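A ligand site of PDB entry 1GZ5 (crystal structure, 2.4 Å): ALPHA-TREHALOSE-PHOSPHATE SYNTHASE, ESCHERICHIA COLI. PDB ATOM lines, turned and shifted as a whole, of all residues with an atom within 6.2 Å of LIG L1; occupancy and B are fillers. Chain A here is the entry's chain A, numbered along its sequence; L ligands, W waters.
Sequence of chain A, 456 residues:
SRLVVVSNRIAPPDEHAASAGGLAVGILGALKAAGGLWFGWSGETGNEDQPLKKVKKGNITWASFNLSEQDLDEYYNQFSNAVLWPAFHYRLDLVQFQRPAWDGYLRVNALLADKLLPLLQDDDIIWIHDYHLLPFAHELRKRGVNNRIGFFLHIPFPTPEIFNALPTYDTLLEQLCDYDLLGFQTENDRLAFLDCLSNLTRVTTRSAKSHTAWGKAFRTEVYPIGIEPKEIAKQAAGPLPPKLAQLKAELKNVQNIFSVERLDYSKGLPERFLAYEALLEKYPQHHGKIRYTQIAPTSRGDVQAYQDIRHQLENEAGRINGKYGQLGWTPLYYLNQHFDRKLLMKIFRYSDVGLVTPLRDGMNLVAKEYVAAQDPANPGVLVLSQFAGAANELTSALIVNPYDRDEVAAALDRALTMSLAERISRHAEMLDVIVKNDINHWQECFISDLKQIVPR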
ATOM      1  N   ASN A   8       5.705 -17.224   9.102  1.00  0.00           N
ATOM      2  CA  ASN A   8       4.289 -16.960   9.097  1.00  0.00           C
ATOM      3  C   ASN A   8       4.048 -15.511   8.676  1.00  0.00           C
ATOM      4  O   ASN A   8       3.380 -15.270   7.654  1.00  0.00           O
ATOM      5  CB  ASN A   8       3.675 -17.258  10.470  1.00  0.00           C
ATOM      6  CG  ASN A   8       2.158 -17.112  10.458  1.00  0.00           C
ATOM      7  OD1 ASN A   8       1.614 -16.151  11.005  1.00  0.00           O
ATOM      8  ND2 ASN A   8       1.484 -18.035   9.776  1.00  0.00           N
ATOM      9  N   ARG A   9       4.626 -14.566   9.434  1.00  0.00           N
ATOM     10  CA  ARG A   9       4.562 -13.144   9.120  1.00  0.00           C
ATOM     11  C   ARG A   9       5.554 -12.798   8.010  1.00  0.00           C
ATOM     12  O   ARG A   9       6.687 -13.302   7.980  1.00  0.00           O
ATOM     13  CB  ARG A   9       4.876 -12.312  10.366  1.00  0.00           C
ATOM     14  CG  ARG A   9       4.583 -10.799  10.278  1.00  0.00           C
ATOM     15  CD  ARG A   9       3.107 -10.483   9.904  1.00  0.00           C
ATOM     16  NE  ARG A   9       2.202 -10.818  10.984  1.00  0.00           N
ATOM     17  CZ  ARG A   9       0.882 -10.688  10.960  1.00  0.00           C
ATOM     18  NH1 ARG A   9       0.233 -10.374   9.844  1.00  0.00           N
ATOM     19  NH2 ARG A   9       0.186 -10.978  12.050  1.00  0.00           N
ATOM     20  N   SER A  19       3.503  -4.233   9.868  1.00  0.00           N
ATOM     21  CA  SER A  19       2.955  -4.465  11.179  1.00  0.00           C
ATOM     22  C   SER A  19       4.197  -4.552  12.087  1.00  0.00           C
ATOM     23  O   SER A  19       5.262  -5.010  11.615  1.00  0.00           O
ATOM     24  CB  SER A  19       2.349  -5.873  11.112  1.00  0.00           C
ATOM     25  OG  SER A  19       1.242  -6.004  11.959  1.00  0.00           O
ATOM     26  N   ALA A  20       4.067  -4.166  13.347  1.00  0.00           N
ATOM     27  CA  ALA A  20       5.170  -4.231  14.289  1.00  0.00           C
ATOM     28  C   ALA A  20       5.603  -5.643  14.411  1.00  0.00           C
ATOM     29  O   ALA A  20       4.779  -6.534  14.311  1.00  0.00           O
ATOM     30  CB  ALA A  20       4.728  -3.738  15.632  1.00  0.00           C
ATOM     31  N   GLY A  21       6.895  -5.844  14.619  1.00  0.00           N
ATOM     32  CA  GLY A  21       7.455  -7.156  14.824  1.00  0.00           C
ATOM     33  C   GLY A  21       8.839  -7.342  14.223  1.00  0.00           C
ATOM     34  O   GLY A  21       9.064  -6.971  13.087  1.00  0.00           O
ATOM     35  N   GLY A  22       9.768  -7.930  14.992  1.00  0.00           N
ATOM     36  CA  GLY A  22      11.169  -7.936  14.657  1.00  0.00           C
ATOM     37  C   GLY A  22      11.512  -8.945  13.586  1.00  0.00           C
ATOM     38  O   GLY A  22      12.461  -8.722  12.768  1.00  0.00           O
ATOM     39  N   LEU A  23      10.785 -10.048  13.578  1.00  0.00           N
ATOM     40  CA  LEU A  23      11.083 -11.114  12.615  1.00  0.00           C
ATOM     41  C   LEU A  23      11.072 -10.590  11.130  1.00  0.00           C
ATOM     42  O   LEU A  23      12.025 -10.766  10.340  1.00  0.00           O
ATOM     43  CB  LEU A  23      10.094 -12.270  12.781  1.00  0.00           C
ATOM     44  CG  LEU A  23      10.109 -13.370  11.696  1.00  0.00           C
ATOM     45  CD1 LEU A  23       9.849 -14.692  12.359  1.00  0.00           C
ATOM     46  CD2 LEU A  23       9.049 -13.078  10.591  1.00  0.00           C
ATOM     47  N   ALA A  24       9.980  -9.931  10.770  1.00  0.00           N
ATOM     48  CA  ALA A  24       9.786  -9.489   9.421  1.00  0.00           C
ATOM     49  C   ALA A  24      10.861  -8.471   9.088  1.00  0.00           C
ATOM     50  O   ALA A  24      11.377  -8.501   7.969  1.00  0.00           O
ATOM     51  CB  ALA A  24       8.381  -8.911   9.236  1.00  0.00           C
ATOM     52  N   TYR A  76      -2.814 -20.209  14.590  1.00  0.00           N
ATOM     53  CA  TYR A  76      -2.209 -18.936  14.918  1.00  0.00           C
ATOM     54  C   TYR A  76      -2.677 -18.427  16.274  1.00  0.00           C
ATOM     55  O   TYR A  76      -1.873 -18.272  17.194  1.00  0.00           O
ATOM     56  CB  TYR A  76      -2.440 -17.912  13.788  1.00  0.00           C
ATOM     57  CG  TYR A  76      -1.900 -16.514  14.064  1.00  0.00           C
ATOM     58  CD1 TYR A  76      -0.518 -16.260  14.034  1.00  0.00           C
ATOM     59  CD2 TYR A  76      -2.761 -15.450  14.280  1.00  0.00           C
ATOM     60  CE1 TYR A  76      -0.018 -14.952  14.241  1.00  0.00           C
ATOM     61  CE2 TYR A  76      -2.300 -14.157  14.505  1.00  0.00           C
ATOM     62  CZ  TYR A  76      -0.916 -13.918  14.501  1.00  0.00           C
ATOM     63  OH  TYR A  76      -0.461 -12.619  14.779  1.00  0.00           O
ATOM     64  N   ASN A  81      -0.001 -18.564  19.407  1.00  0.00           N
ATOM     65  CA  ASN A  81      -0.105 -17.405  20.293  1.00  0.00           C
ATOM     66  C   ASN A  81      -0.589 -17.677  21.749  1.00  0.00           C
ATOM     67  O   ASN A  81      -0.343 -16.831  22.596  1.00  0.00           O
ATOM     68  CB  ASN A  81      -1.029 -16.337  19.675  1.00  0.00           C
ATOM     69  CG  ASN A  81      -0.481 -15.765  18.366  1.00  0.00           C
ATOM     70  OD1 ASN A  81       0.690 -15.932  18.009  1.00  0.00           O
ATOM     71  ND2 ASN A  81      -1.370 -15.083  17.620  1.00  0.00           N
ATOM     72  N   TRP A  85       3.891 -19.237  22.298  1.00  0.00           N
ATOM     73  CA  TRP A  85       4.399 -17.927  22.721  1.00  0.00           C
ATOM     74  C   TRP A  85       4.456 -17.796  24.279  1.00  0.00           C
ATOM     75  O   TRP A  85       5.540 -17.513  24.810  1.00  0.00           O
ATOM     76  CB  TRP A  85       3.608 -16.780  22.114  1.00  0.00           C
ATOM     77  CG  TRP A  85       4.139 -15.446  22.588  1.00  0.00           C
ATOM     78  CD1 TRP A  85       3.750 -14.739  23.661  1.00  0.00           C
ATOM     79  CD2 TRP A  85       5.183 -14.670  21.959  1.00  0.00           C
ATOM     80  NE1 TRP A  85       4.468 -13.587  23.764  1.00  0.00           N
ATOM     81  CE2 TRP A  85       5.354 -13.508  22.728  1.00  0.00           C
ATOM     82  CE3 TRP A  85       5.979 -14.847  20.791  1.00  0.00           C
ATOM     83  CZ2 TRP A  85       6.295 -12.494  22.393  1.00  0.00           C
ATOM     84  CZ3 TRP A  85       6.903 -13.852  20.446  1.00  0.00           C
ATOM     85  CH2 TRP A  85       7.050 -12.689  21.232  1.00  0.00           C
ATOM     86  N   HIS A 129      11.499 -20.126   9.658  1.00  0.00           N
ATOM     87  CA  HIS A 129      11.585 -19.234  10.801  1.00  0.00           C
ATOM     88  C   HIS A 129      10.408 -19.313  11.762  1.00  0.00           C
ATOM     89  O   HIS A 129       9.233 -19.106  11.385  1.00  0.00           O
ATOM     90  CB  HIS A 129      11.668 -17.757  10.327  1.00  0.00           C
ATOM     91  CG  HIS A 129      12.938 -17.440   9.645  1.00  0.00           C
ATOM     92  ND1 HIS A 129      13.984 -16.820  10.288  1.00  0.00           N
ATOM     93  CD2 HIS A 129      13.351 -17.709   8.381  1.00  0.00           C
ATOM     94  CE1 HIS A 129      14.984 -16.675   9.436  1.00  0.00           C
ATOM     95  NE2 HIS A 129      14.626 -17.223   8.277  1.00  0.00           N
ATOM     96  N   ASP A 130      10.779 -19.558  13.017  1.00  0.00           N
ATOM     97  CA  ASP A 130      10.004 -19.219  14.203  1.00  0.00           C
ATOM     98  C   ASP A 130       8.995 -20.269  14.625  1.00  0.00           C
ATOM     99  O   ASP A 130       8.774 -21.275  13.909  1.00  0.00           O
ATOM    100  CB  ASP A 130       9.397 -17.828  14.140  1.00  0.00           C
ATOM    101  CG  ASP A 130       9.701 -17.024  15.397  1.00  0.00           C
ATOM    102  OD1 ASP A 130      10.454 -17.592  16.268  1.00  0.00           O
ATOM    103  OD2 ASP A 130       9.249 -15.849  15.630  1.00  0.00           O
ATOM    104  N   TYR A 131       8.396 -20.031  15.790  1.00  0.00           N
ATOM    105  CA  TYR A 131       7.668 -21.042  16.540  1.00  0.00           C
ATOM    106  C   TYR A 131       6.395 -21.495  15.858  1.00  0.00           C
ATOM    107  O   TYR A 131       5.873 -22.526  16.202  1.00  0.00           O
ATOM    108  CB  TYR A 131       7.321 -20.513  17.908  1.00  0.00           C
ATOM    109  CG  TYR A 131       6.619 -19.144  17.870  1.00  0.00           C
ATOM    110  CD1 TYR A 131       7.370 -17.976  17.751  1.00  0.00           C
ATOM    111  CD2 TYR A 131       5.238 -19.039  17.861  1.00  0.00           C
ATOM    112  CE1 TYR A 131       6.784 -16.763  17.706  1.00  0.00           C
ATOM    113  CE2 TYR A 131       4.643 -17.806  17.813  1.00  0.00           C
ATOM    114  CZ  TYR A 131       5.431 -16.673  17.737  1.00  0.00           C
ATOM    115  OH  TYR A 131       4.859 -15.413  17.695  1.00  0.00           O
ATOM    116  N   HIS A 132       5.914 -20.756  14.861  1.00  0.00           N
ATOM    117  CA  HIS A 132       4.767 -21.259  14.102  1.00  0.00           C
ATOM    118  C   HIS A 132       5.090 -22.519  13.357  1.00  0.00           C
ATOM    119  O   HIS A 132       4.187 -23.292  13.003  1.00  0.00           O
ATOM    120  CB  HIS A 132       4.275 -20.193  13.114  1.00  0.00           C
ATOM    121  CG  HIS A 132       4.173 -18.836  13.728  1.00  0.00           C
ATOM    122  ND1 HIS A 132       5.254 -18.001  13.855  1.00  0.00           N
ATOM    123  CD2 HIS A 132       3.105 -18.167  14.243  1.00  0.00           C
ATOM    124  CE1 HIS A 132       4.865 -16.872  14.422  1.00  0.00           C
ATOM    125  NE2 HIS A 132       3.570 -16.940  14.683  1.00  0.00           N
ATOM    126  N   HIS A 154      13.212 -17.236  16.750  1.00  0.00           N
ATOM    127  CA  HIS A 154      13.412 -15.837  17.030  1.00  0.00           C
ATOM    128  C   HIS A 154      13.182 -15.515  18.505  1.00  0.00           C
ATOM    129  O   HIS A 154      13.472 -14.417  18.963  1.00  0.00           O
ATOM    130  CB  HIS A 154      12.445 -15.056  16.146  1.00  0.00           C
ATOM    131  CG  HIS A 154      12.856 -15.041  14.706  1.00  0.00           C
ATOM    132  ND1 HIS A 154      13.371 -13.915  14.070  1.00  0.00           N
ATOM    133  CD2 HIS A 154      12.903 -16.048  13.778  1.00  0.00           C
ATOM    134  CE1 HIS A 154      13.651 -14.216  12.804  1.00  0.00           C
ATOM    135  NE2 HIS A 154      13.410 -15.498  12.619  1.00  0.00           N
ATOM    136  N   ILE A 155      12.640 -16.461  19.243  1.00  0.00           N
ATOM    137  CA  ILE A 155      12.189 -16.225  20.594  1.00  0.00           C
ATOM    138  C   ILE A 155      12.963 -17.157  21.530  1.00  0.00           C
ATOM    139  O   ILE A 155      13.735 -17.930  21.073  1.00  0.00           O
ATOM    140  CB  ILE A 155      10.651 -16.465  20.721  1.00  0.00           C
ATOM    141  CG1 ILE A 155      10.273 -17.922  20.503  1.00  0.00           C
ATOM    142  CG2 ILE A 155       9.859 -15.508  19.804  1.00  0.00           C
ATOM    143  CD1 ILE A 155       8.826 -18.173  20.868  1.00  0.00           C
ATOM    144  N   ARG A 262       5.256  -3.856  20.425  1.00  0.00           N
ATOM    145  CA  ARG A 262       3.940  -4.496  20.449  1.00  0.00           C
ATOM    146  C   ARG A 262       3.417  -4.580  21.879  1.00  0.00           C
ATOM    147  O   ARG A 262       4.155  -4.830  22.839  1.00  0.00           O
ATOM    148  CB  ARG A 262       4.019  -5.911  19.849  1.00  0.00           C
ATOM    149  CG  ARG A 262       4.297  -5.988  18.325  1.00  0.00           C
ATOM    150  CD  ARG A 262       4.436  -7.491  17.833  1.00  0.00           C
ATOM    151  NE  ARG A 262       5.398  -8.197  18.641  1.00  0.00           N
ATOM    152  CZ  ARG A 262       5.085  -9.038  19.648  1.00  0.00           C
ATOM    153  NH1 ARG A 262       3.811  -9.358  19.896  1.00  0.00           N
ATOM    154  NH2 ARG A 262       6.081  -9.592  20.375  1.00  0.00           N
ATOM    155  N   SER A 299      -1.349  -6.023  19.479  1.00  0.00           N
ATOM    156  CA  SER A 299      -0.811  -7.171  18.797  1.00  0.00           C
ATOM    157  C   SER A 299      -1.686  -8.358  19.200  1.00  0.00           C
ATOM    158  O   SER A 299      -1.963  -8.483  20.394  1.00  0.00           O
ATOM    159  CB  SER A 299       0.613  -7.399  19.301  1.00  0.00           C
ATOM    160  OG  SER A 299       1.158  -8.590  18.751  1.00  0.00           O
ATOM    161  N   ARG A 300      -2.132  -9.187  18.266  1.00  0.00           N
ATOM    162  CA  ARG A 300      -2.777 -10.471  18.609  1.00  0.00           C
ATOM    163  C   ARG A 300      -3.984 -10.226  19.497  1.00  0.00           C
ATOM    164  O   ARG A 300      -4.180 -10.930  20.491  1.00  0.00           O
ATOM    165  CB  ARG A 300      -1.755 -11.383  19.344  1.00  0.00           C
ATOM    166  CG  ARG A 300      -0.554 -11.788  18.464  1.00  0.00           C
ATOM    167  CD  ARG A 300       0.585 -12.422  19.184  1.00  0.00           C
ATOM    168  NE  ARG A 300       1.799 -12.352  18.412  1.00  0.00           N
ATOM    169  CZ  ARG A 300       3.016 -12.638  18.910  1.00  0.00           C
ATOM    170  NH1 ARG A 300       3.155 -13.064  20.183  1.00  0.00           N
ATOM    171  NH2 ARG A 300       4.082 -12.542  18.141  1.00  0.00           N
HETATM  172  C1  LIG L   1       7.699 -11.687  17.089  1.00  0.00           C
HETATM  173  C2  LIG L   1       7.707 -13.111  16.569  1.00  0.00           C
HETATM  174  C3  LIG L   1       7.415 -13.134  15.058  1.00  0.00           C
HETATM  175  C4  LIG L   1       6.145 -12.335  14.861  1.00  0.00           C
HETATM  176  C5  LIG L   1       6.275 -10.934  15.391  1.00  0.00           C
HETATM  177  C6  LIG L   1       4.971 -10.193  15.266  1.00  0.00           C
HETATM  178  O1  LIG L   1       8.686 -10.965  16.506  1.00  0.00           O
HETATM  179  O2  LIG L   1       8.992 -13.602  16.882  1.00  0.00           O
HETATM  180  O3  LIG L   1       7.166 -14.493  14.627  1.00  0.00           O
HETATM  181  O4  LIG L   1       5.780 -12.265  13.507  1.00  0.00           O
HETATM  182  O5  LIG L   1       6.470 -11.053  16.812  1.00  0.00           O
HETATM  183  O6  LIG L   1       3.833 -10.977  15.620  1.00  0.00           O
HETATM  184  P1  LIG L   1       2.621 -11.408  14.617  1.00  0.00           P
HETATM  185  O7  LIG L   1       1.756 -10.224  14.415  1.00  0.00           O
HETATM  186  O8  LIG L   1       1.930 -12.409  15.441  1.00  0.00           O
HETATM  187  O9  LIG L   1       3.407 -11.952  13.438  1.00  0.00           O
HETATM  188  N1  LG2 L   2       7.998  -1.481  15.364  1.00  0.00           N
HETATM  189  C1  LG2 L   2       7.400  -0.680  14.405  1.00  0.00           C
HETATM  190  N2  LG2 L   2       6.300   0.130  14.699  1.00  0.00           N
HETATM  191  C2  LG2 L   2       5.787   0.094  15.980  1.00  0.00           C
HETATM  192  C3  LG2 L   2       6.340  -0.775  16.952  1.00  0.00           C
HETATM  193  C4  LG2 L   2       7.437  -1.587  16.627  1.00  0.00           C
HETATM  194  O1  LG2 L   2       7.906  -0.690  13.283  1.00  0.00           O
HETATM  195  O2  LG2 L   2       4.790   0.797  16.211  1.00  0.00           O
HETATM  196  C5  LG2 L   2       9.090  -2.279  14.883  1.00  0.00           C
HETATM  197  C6  LG2 L   2      10.298  -1.935  15.652  1.00  0.00           C
HETATM  198  O3  LG2 L   2      10.893  -0.810  15.081  1.00  0.00           O
HETATM  199  C7  LG2 L   2      11.086  -3.213  15.526  1.00  0.00           C
HETATM  200  C8  LG2 L   2      10.023  -4.281  15.566  1.00  0.00           C
HETATM  201  O4  LG2 L   2       8.808  -3.613  15.219  1.00  0.00           O
HETATM  202  O5  LG2 L   2      11.820  -3.306  14.317  1.00  0.00           O
HETATM  203  C9  LG2 L   2       9.932  -4.816  17.009  1.00  0.00           C
HETATM  204  O6  LG2 L   2      10.807  -5.904  17.047  1.00  0.00           O
HETATM  205  P1  LG2 L   2      11.387  -6.326  18.470  1.00  0.00           P
HETATM  206  O7  LG2 L   2      12.488  -7.264  18.304  1.00  0.00           O
HETATM  207  O8  LG2 L   2      11.712  -5.206  19.390  1.00  0.00           O
HETATM  208  O9  LG2 L   2      10.105  -6.955  19.233  1.00  0.00           O
HETATM  209  P2  LG2 L   2       9.113  -8.042  18.722  1.00  0.00           P
HETATM  210  O10 LG2 L   2       9.637  -8.818  17.576  1.00  0.00           O
HETATM  211  O11 LG2 L   2       7.865  -7.406  18.220  1.00  0.00           O
HETATM  212  O12 LG2 L   2       8.746  -8.815  19.943  1.00  0.00           O
HETATM  213  O   HOH W   1       2.564 -14.958  16.323  1.00  0.00           O
HETATM  214  O   HOH W   2       3.286 -14.565  12.986  1.00  0.00           O
HETATM  215  O   HOH W   3       6.221 -14.993  11.927  1.00  0.00           O
HETATM  216  O   HOH W   4       1.079  -8.418  16.273  1.00  0.00           O
HETATM  217  O   HOH W   5       2.649  -8.048  12.960  1.00  0.00           O
HETATM  218  O   HOH W   6       7.259  -9.875  12.385  1.00  0.00           O
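The backbone carbonyl oxygen (O) of Tyr 76 lies within hydrogen-bond range of the backbone NH (N) of Asn 81, at 2.9 Å.
OD1 of Asp 130 is in hydrogen-bond range of N of His 154, 2.8 Å away.
OH of Tyr 131 is in hydrogen-bond range of NH2 of Arg 300.
A ring nitrogen (NE2) of His 154 lies within hydrogen-bond range of a ring nitrogen (ND1) of His 129 (2.7 Å).
OH of Tyr 76 is in hydrogen-bond range of NH2 of Arg 9, at 3.2 Å.
The guanidinium group (NH1) of Arg 262 sits at hydrogen-bond distance from the side-chain hydroxyl (OG) of Ser 299.
O10 of LG2 L2 is in hydrogen-bond range of O1 of LIG L1, at 2.6 Å.
Residues that only touch LIG L1: Ala 20 (3.8 Å), Gly 21 (3.9 Å), Gly 22 (3.6 Å), Leu 23 (3.5 Å), Tyr 131 (3.8 Å), His 132 (3.3 Å), His 154 (3.8 Å), Ile 155 (3.6 Å) and Arg 262 (3.6 Å).
Hydrophobic or aromatic side chains that line LIG L1: Leu 23, Tyr 76, Tyr 131, His 132, His 154 and Ile 155.
Of the 20 residues printed, 13 come within 4 Å of LIG L1.
The nearest printed residue that does not touch LIG L1 is Trp 85 (4.03 Å).
NE of Arg 300 is in salt-bridge range of O8 of LIG L1 (3.0 Å).
NE of Arg 262 lies within salt-bridge range of O11 of LG2 L2 (2.6 Å).
The side-chain carboxylate of Asp 130 lies within hydrogen-bond range of an oxygen (O2) of LIG L1, 2.6 Å away.
N of Gly 22 lies within hydrogen-bond range of O10 of LG2 L2, at 2.7 Å.
An oxygen (O7) of LIG L1 lies within salt-bridge range of the guanidinium group of Arg 9 (2.9 Å).
The backbone NH (N) of Gly 21 is in hydrogen-bond range of an oxygen (O4) of LG2 L2, 3.0 Å away.
The side-chain hydroxyl (OH) of Tyr 76 is in hydrogen-bond range of an oxygen (O8) of LIG L1, 2.5 Å away.
Water W2 lies within hydrogen-bond range of an oxygen (O9) of LIG L1 (2.7 Å), a ring nitrogen (NE2) of His 132 (2.9 Å) and the side-chain amide oxygen (OD1) of Asn 8 (3.0 Å).
Water W4 bridges the side-chain hydroxyl (OG) of Ser 299 (2.5 Å) and an oxygen (O7) of LIG L1 (2.7 Å).
Water W5 lies within hydrogen-bond range of OG of Ser 19 (2.7 Å), O7 of LIG L1 (2.8 Å), O of Ala 20 (2.9 Å) and NE of Arg 9 (3.4 Å).
Water W1 lies within hydrogen-bond range of the side-chain amide oxygen (OD1) of Asn 81, the side-chain hydroxyl (OH) of Tyr 131, a ring nitrogen (NE2) of His 132, an oxygen (O8) of LIG L1 and the guanidinium group (NH2) of Arg 300.
Water W3 bridges O3 of LIG L1 (2.9 Å) and N of Arg 9 (3.0 Å).
Water W6 lies within hydrogen-bond range of an oxygen (O4) of LIG L1 (3.0 Å), the backbone NH (N) of Ala 24 (3.2 Å) and the backbone carbonyl oxygen (O) of Gly 21 (3.5 Å).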
